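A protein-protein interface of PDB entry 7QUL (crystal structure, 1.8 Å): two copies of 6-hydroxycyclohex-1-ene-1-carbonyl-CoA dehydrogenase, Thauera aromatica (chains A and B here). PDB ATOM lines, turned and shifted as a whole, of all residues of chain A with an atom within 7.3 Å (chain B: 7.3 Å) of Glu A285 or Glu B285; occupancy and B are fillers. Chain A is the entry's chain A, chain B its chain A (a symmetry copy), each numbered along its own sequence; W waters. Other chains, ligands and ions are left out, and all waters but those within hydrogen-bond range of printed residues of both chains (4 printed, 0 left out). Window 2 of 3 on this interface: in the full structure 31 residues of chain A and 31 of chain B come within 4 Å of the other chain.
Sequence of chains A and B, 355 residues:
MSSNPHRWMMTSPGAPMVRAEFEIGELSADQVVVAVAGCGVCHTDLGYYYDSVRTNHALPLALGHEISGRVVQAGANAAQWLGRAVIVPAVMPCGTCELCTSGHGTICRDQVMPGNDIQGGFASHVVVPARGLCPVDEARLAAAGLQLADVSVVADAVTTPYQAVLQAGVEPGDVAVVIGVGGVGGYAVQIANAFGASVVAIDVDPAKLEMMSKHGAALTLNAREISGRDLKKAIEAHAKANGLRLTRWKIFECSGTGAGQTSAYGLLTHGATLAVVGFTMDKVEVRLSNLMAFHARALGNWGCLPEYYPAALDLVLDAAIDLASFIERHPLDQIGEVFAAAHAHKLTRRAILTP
Among the printed residues, merely in contact across the chains: Lys A283 with Val B286 (3.4 Å), Lys A283 with Arg B287 (3.7 Å), Val A284 with Val B284 (3.6 Å), Val A284 with Glu B285 (3.4 Å), Glu A285 with Val B284 (3.4 Å), Val A286 with Lys B283 (3.4 Å) and Arg A287 with Lys B283 (3.7 Å).
Printed residues of chain B within 4 Å of Lys A283: Val B286 and Arg B287. Glu A285 touches two residues of chain B. Of the printed residues of chain B, Val A286 touches Lys B283 (3.4 Å) and Val B284 (3.1 Å). Leu A288 touches none of the printed residues of chain B. Tyr B265 touches none of the printed residues of chain A. Of chain A, only Val A284 and Glu A285 come within 4 Å of Glu B285. Of the printed residues of chain A, Val B286 touches Lys A283 and Val A284. The nearest printed residue of chain B that does not touch Arg A287 is Val B284 (5.0 Å).
O of Arg B287 is in hydrogen-bond range of OH of Tyr B265, 2.8 Å away. O of Arg A287 lies within hydrogen-bond range of OH of Tyr A265, at 2.8 Å.
Water W3 lies within hydrogen-bond range of the backbone NH (N) of Leu B288 (2.8 Å), the backbone carbonyl oxygen (O) of Val B286 (3.3 Å) and the backbone NH (N) of Val A284 (3.5 Å). Water W1 lies within hydrogen-bond range of the backbone NH (N) of Leu A288, the backbone carbonyl oxygen (O) of Val A286 and the backbone NH (N) of Val B284. Water W4 lies within hydrogen-bond range of NZ of Lys A283 (3.2 Å) and NH2 of Arg B287 (3.4 Å). Water W2 bridges NZ of Lys B283 (3.2 Å) and NH2 of Arg A287 (3.4 Å).
Of the 9 printed residues of chain B, 5 touch a printed residue of chain A. Hydrophobic or aromatic side chains of chain B within 4 Å of the printed part of chain A: Val B284. Printed residues of chain A that touch a printed residue of chain B: Lys A283, Val A284, Glu A285, Val A286 and Arg A287. Along chain A the printed residues that touch a printed residue of chain B span positions 283 to 287.
Lys A283 touches Val B286, and with the chains exchanged Val A286 touches Lys B283. Val B284 touches its own counterpart, Val A284. Val A284 touches Glu B285, and with the chains exchanged Glu A285 touches Val B284. Val A284 touches Val B286, and with the chains exchanged Val A286 touches Val B284. Positions printed for both chains: 258, 262, 265, 283, 284, 285, 286, 287 and 288.
OE2 of Glu A285 lies close to OE2 of Glu B285. The backbone NH of Val A284 is in hydrogen-bond range of the backbone carbonyl oxygen of Val B286 (3.1 Å). The backbone NH (N) of Val B284 is in hydrogen-bond range of the backbone carbonyl oxygen (O) of Val A286.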
ATOM      1  N   GLY A 258      -9.975 -30.560  -7.984  1.00  0.00           N
ATOM      2  CA  GLY A 258     -10.817 -29.364  -8.156  1.00  0.00           C
ATOM      3  C   GLY A 258     -10.586 -28.687  -9.500  1.00  0.00           C
ATOM      4  O   GLY A 258     -11.574 -28.290 -10.137  1.00  0.00           O
ATOM      5  N   THR A 262     -13.675 -28.232 -12.048  1.00  0.00           N
ATOM      6  CA  THR A 262     -14.009 -26.883 -12.579  1.00  0.00           C
ATOM      7  C   THR A 262     -14.040 -26.912 -14.104  1.00  0.00           C
ATOM      8  O   THR A 262     -15.008 -26.398 -14.687  1.00  0.00           O
ATOM      9  CB  THR A 262     -12.999 -25.844 -12.082  1.00  0.00           C
ATOM     10  OG1 THR A 262     -13.288 -25.733 -10.695  1.00  0.00           O
ATOM     11  CG2 THR A 262     -13.136 -24.508 -12.776  1.00  0.00           C
ATOM     12  N   TYR A 265     -16.902 -29.251 -15.541  1.00  0.00           N
ATOM     13  CA  TYR A 265     -18.197 -28.556 -15.273  1.00  0.00           C
ATOM     14  C   TYR A 265     -18.359 -27.416 -16.275  1.00  0.00           C
ATOM     15  O   TYR A 265     -19.465 -27.205 -16.834  1.00  0.00           O
ATOM     16  CB  TYR A 265     -18.291 -27.996 -13.856  1.00  0.00           C
ATOM     17  CG  TYR A 265     -19.701 -27.717 -13.421  1.00  0.00           C
ATOM     18  CD1 TYR A 265     -20.471 -28.717 -12.856  1.00  0.00           C
ATOM     19  CD2 TYR A 265     -20.278 -26.463 -13.589  1.00  0.00           C
ATOM     20  CE1 TYR A 265     -21.791 -28.490 -12.497  1.00  0.00           C
ATOM     21  CE2 TYR A 265     -21.580 -26.214 -13.190  1.00  0.00           C
ATOM     22  CZ  TYR A 265     -22.358 -27.244 -12.699  1.00  0.00           C
ATOM     23  OH  TYR A 265     -23.644 -27.022 -12.285  1.00  0.00           O
ATOM     24  N   LYS A 283     -13.319 -29.190  -2.462  1.00  0.00           N
ATOM     25  CA  LYS A 283     -14.605 -28.551  -2.850  1.00  0.00           C
ATOM     26  C   LYS A 283     -14.318 -27.599  -4.011  1.00  0.00           C
ATOM     27  O   LYS A 283     -13.230 -27.019  -4.045  1.00  0.00           O
ATOM     28  CB  LYS A 283     -15.250 -27.847  -1.649  1.00  0.00           C
ATOM     29  CG  LYS A 283     -15.564 -28.749  -0.466  1.00  0.00           C
ATOM     30  CD  LYS A 283     -16.101 -27.997   0.734  1.00  0.00           C
ATOM     31  CE  LYS A 283     -16.454 -28.913   1.881  1.00  0.00           C
ATOM     32  NZ  LYS A 283     -17.084 -28.164   2.992  1.00  0.00           N
ATOM     33  N   VAL A 284     -15.236 -27.509  -4.965  1.00  0.00           N
ATOM     34  CA  VAL A 284     -15.168 -26.549  -6.101  1.00  0.00           C
ATOM     35  C   VAL A 284     -16.292 -25.535  -5.894  1.00  0.00           C
ATOM     36  O   VAL A 284     -17.196 -25.815  -5.076  1.00  0.00           O
ATOM     37  CB  VAL A 284     -15.267 -27.225  -7.483  1.00  0.00           C
ATOM     38  CG1 VAL A 284     -13.973 -27.921  -7.875  1.00  0.00           C
ATOM     39  CG2 VAL A 284     -16.438 -28.189  -7.587  1.00  0.00           C
ATOM     40  N   GLU A 285     -16.182 -24.396  -6.586  1.00  0.00           N
ATOM     41  CA  GLU A 285     -17.222 -23.347  -6.730  1.00  0.00           C
ATOM     42  C   GLU A 285     -17.824 -23.464  -8.130  1.00  0.00           C
ATOM     43  O   GLU A 285     -17.091 -23.281  -9.128  1.00  0.00           O
ATOM     44  CB  GLU A 285     -16.640 -21.953  -6.489  1.00  0.00           C
ATOM     45  CG  GLU A 285     -16.739 -21.520  -5.039  1.00  0.00           C
ATOM     46  CD  GLU A 285     -16.626 -20.022  -4.804  1.00  0.00           C
ATOM     47  OE1 GLU A 285     -16.773 -19.249  -5.775  1.00  0.00           O
ATOM     48  OE2 GLU A 285     -16.390 -19.636  -3.644  1.00  0.00           O
ATOM     49  N   VAL A 286     -19.110 -23.805  -8.194  1.00  0.00           N
ATOM     50  CA  VAL A 286     -19.866 -23.960  -9.463  1.00  0.00           C
ATOM     51  C   VAL A 286     -21.287 -23.459  -9.215  1.00  0.00           C
ATOM     52  O   VAL A 286     -21.764 -23.574  -8.059  1.00  0.00           O
ATOM     53  CB  VAL A 286     -19.868 -25.424  -9.950  1.00  0.00           C
ATOM     54  CG1 VAL A 286     -18.475 -25.909 -10.310  1.00  0.00           C
ATOM     55  CG2 VAL A 286     -20.527 -26.359  -8.953  1.00  0.00           C
ATOM     56  N   ARG A 287     -21.959 -22.956 -10.250  1.00  0.00           N
ATOM     57  CA  ARG A 287     -23.414 -22.711 -10.105  1.00  0.00           C
ATOM     58  C   ARG A 287     -24.111 -23.988 -10.567  1.00  0.00           C
ATOM     59  O   ARG A 287     -23.999 -24.337 -11.771  1.00  0.00           O
ATOM     60  CB  ARG A 287     -23.863 -21.387 -10.731  1.00  0.00           C
ATOM     61  CG  ARG A 287     -23.759 -21.276 -12.239  1.00  0.00           C
ATOM     62  CD  ARG A 287     -24.419 -19.978 -12.681  1.00  0.00           C
ATOM     63  NE  ARG A 287     -23.511 -19.162 -13.483  1.00  0.00           N
ATOM     64  CZ  ARG A 287     -22.803 -18.113 -13.055  1.00  0.00           C
ATOM     65  NH1 ARG A 287     -22.888 -17.677 -11.807  1.00  0.00           N
ATOM     66  NH2 ARG A 287     -22.004 -17.493 -13.902  1.00  0.00           N
ATOM     67  N   LEU A 288     -24.675 -24.693  -9.584  1.00  0.00           N
ATOM     68  CA  LEU A 288     -25.492 -25.918  -9.747  1.00  0.00           C
ATOM     69  C   LEU A 288     -26.543 -25.684 -10.842  1.00  0.00           C
ATOM     70  O   LEU A 288     -26.906 -26.661 -11.501  1.00  0.00           O
ATOM     71  CB  LEU A 288     -26.116 -26.277  -8.395  1.00  0.00           C
ATOM     72  N   GLY B 258     -28.387 -20.431  -3.062  1.00  0.00           N
ATOM     73  CA  GLY B 258     -27.184 -21.124  -2.572  1.00  0.00           C
ATOM     74  C   GLY B 258     -27.420 -21.806  -1.232  1.00  0.00           C
ATOM     75  O   GLY B 258     -26.968 -22.951  -1.066  1.00  0.00           O
ATOM     76  N   THR B 262     -26.863 -25.785  -0.909  1.00  0.00           N
ATOM     77  CA  THR B 262     -25.949 -26.326   0.133  1.00  0.00           C
ATOM     78  C   THR B 262     -26.679 -27.356   0.989  1.00  0.00           C
ATOM     79  O   THR B 262     -26.124 -28.444   1.210  1.00  0.00           O
ATOM     80  CB  THR B 262     -25.399 -25.194   1.006  1.00  0.00           C
ATOM     81  OG1 THR B 262     -24.525 -24.491   0.133  1.00  0.00           O
ATOM     82  CG2 THR B 262     -24.661 -25.696   2.227  1.00  0.00           C
ATOM     83  N   TYR B 265     -27.798 -30.555  -1.070  1.00  0.00           N
ATOM     84  CA  TYR B 265     -26.553 -31.319  -1.382  1.00  0.00           C
ATOM     85  C   TYR B 265     -26.098 -32.051  -0.123  1.00  0.00           C
ATOM     86  O   TYR B 265     -25.695 -33.241  -0.182  1.00  0.00           O
ATOM     87  CB  TYR B 265     -25.418 -30.431  -1.885  1.00  0.00           C
ATOM     88  CG  TYR B 265     -24.353 -31.190  -2.623  1.00  0.00           C
ATOM     89  CD1 TYR B 265     -24.481 -31.440  -3.977  1.00  0.00           C
ATOM     90  CD2 TYR B 265     -23.226 -31.679  -1.973  1.00  0.00           C
ATOM     91  CE1 TYR B 265     -23.533 -32.184  -4.663  1.00  0.00           C
ATOM     92  CE2 TYR B 265     -22.250 -32.382  -2.658  1.00  0.00           C
ATOM     93  CZ  TYR B 265     -22.433 -32.687  -3.992  1.00  0.00           C
ATOM     94  OH  TYR B 265     -21.478 -33.370  -4.696  1.00  0.00           O
ATOM     95  N   LYS B 283     -23.203 -19.240  -6.967  1.00  0.00           N
ATOM     96  CA  LYS B 283     -22.315 -20.433  -6.928  1.00  0.00           C
ATOM     97  C   LYS B 283     -22.283 -20.940  -5.488  1.00  0.00           C
ATOM     98  O   LYS B 283     -22.365 -20.121  -4.569  1.00  0.00           O
ATOM     99  CB  LYS B 283     -20.921 -20.094  -7.471  1.00  0.00           C
ATOM    100  CG  LYS B 283     -20.893 -19.590  -8.905  1.00  0.00           C
ATOM    101  CD  LYS B 283     -19.512 -19.168  -9.364  1.00  0.00           C
ATOM    102  CE  LYS B 283     -19.493 -18.718 -10.805  1.00  0.00           C
ATOM    103  NZ  LYS B 283     -18.114 -18.425 -11.259  1.00  0.00           N
ATOM    104  N   VAL B 284     -22.245 -22.255  -5.306  1.00  0.00           N
ATOM    105  CA  VAL B 284     -22.094 -22.910  -3.977  1.00  0.00           C
ATOM    106  C   VAL B 284     -20.717 -23.573  -3.963  1.00  0.00           C
ATOM    107  O   VAL B 284     -20.124 -23.724  -5.054  1.00  0.00           O
ATOM    108  CB  VAL B 284     -23.211 -23.926  -3.664  1.00  0.00           C
ATOM    109  CG1 VAL B 284     -24.515 -23.244  -3.280  1.00  0.00           C
ATOM    110  CG2 VAL B 284     -23.445 -24.915  -4.794  1.00  0.00           C
ATOM    111  N   GLU B 285     -20.241 -23.896  -2.756  1.00  0.00           N
ATOM    112  CA  GLU B 285     -19.043 -24.726  -2.473  1.00  0.00           C
ATOM    113  C   GLU B 285     -19.518 -26.106  -2.019  1.00  0.00           C
ATOM    114  O   GLU B 285     -20.190 -26.205  -0.968  1.00  0.00           O
ATOM    115  CB  GLU B 285     -18.151 -24.068  -1.418  1.00  0.00           C
ATOM    116  CG  GLU B 285     -17.093 -23.167  -2.027  1.00  0.00           C
ATOM    117  CD  GLU B 285     -15.909 -22.862  -1.123  1.00  0.00           C
ATOM    118  OE1 GLU B 285     -15.721 -23.578  -0.116  1.00  0.00           O
ATOM    119  OE2 GLU B 285     -15.178 -21.903  -1.434  1.00  0.00           O
ATOM    120  N   VAL B 286     -19.211 -27.128  -2.815  1.00  0.00           N
ATOM    121  CA  VAL B 286     -19.581 -28.539  -2.535  1.00  0.00           C
ATOM    122  C   VAL B 286     -18.434 -29.420  -3.023  1.00  0.00           C
ATOM    123  O   VAL B 286     -17.752 -29.021  -3.999  1.00  0.00           O
ATOM    124  CB  VAL B 286     -20.910 -28.926  -3.217  1.00  0.00           C
ATOM    125  CG1 VAL B 286     -22.086 -28.140  -2.666  1.00  0.00           C
ATOM    126  CG2 VAL B 286     -20.836 -28.805  -4.728  1.00  0.00           C
ATOM    127  N   ARG B 287     -18.238 -30.585  -2.406  1.00  0.00           N
ATOM    128  CA  ARG B 287     -17.315 -31.570  -3.019  1.00  0.00           C
ATOM    129  C   ARG B 287     -18.172 -32.454  -3.921  1.00  0.00           C
ATOM    130  O   ARG B 287     -19.055 -33.180  -3.395  1.00  0.00           O
ATOM    131  CB  ARG B 287     -16.411 -32.262  -1.993  1.00  0.00           C
ATOM    132  CG  ARG B 287     -17.090 -33.173  -0.990  1.00  0.00           C
ATOM    133  CD  ARG B 287     -16.021 -33.903  -0.189  1.00  0.00           C
ATOM    134  NE  ARG B 287     -16.208 -33.714   1.247  1.00  0.00           N
ATOM    135  CZ  ARG B 287     -15.543 -32.854   2.024  1.00  0.00           C
ATOM    136  NH1 ARG B 287     -14.585 -32.075   1.543  1.00  0.00           N
ATOM    137  NH2 ARG B 287     -15.847 -32.785   3.307  1.00  0.00           N
ATOM    138  N   LEU B 288     -17.975 -32.261  -5.227  1.00  0.00           N
ATOM    139  CA  LEU B 288     -18.596 -33.036  -6.327  1.00  0.00           C
ATOM    140  C   LEU B 288     -18.455 -34.536  -6.031  1.00  0.00           C
ATOM    141  O   LEU B 288     -19.334 -35.286  -6.462  1.00  0.00           O
ATOM    142  CB  LEU B 288     -17.937 -32.628  -7.648  1.00  0.00           C
HETATM  143  O   HOH W   1     -24.938 -23.076  -7.302  1.00  0.00           O
HETATM  144  O   HOH W   2     -18.718 -18.370 -14.358  1.00  0.00           O
HETATM  145  O   HOH W   3     -15.559 -30.883  -5.617  1.00  0.00           O
HETATM  146  O   HOH W   4     -18.234 -30.658   4.552  1.00  0.00           O
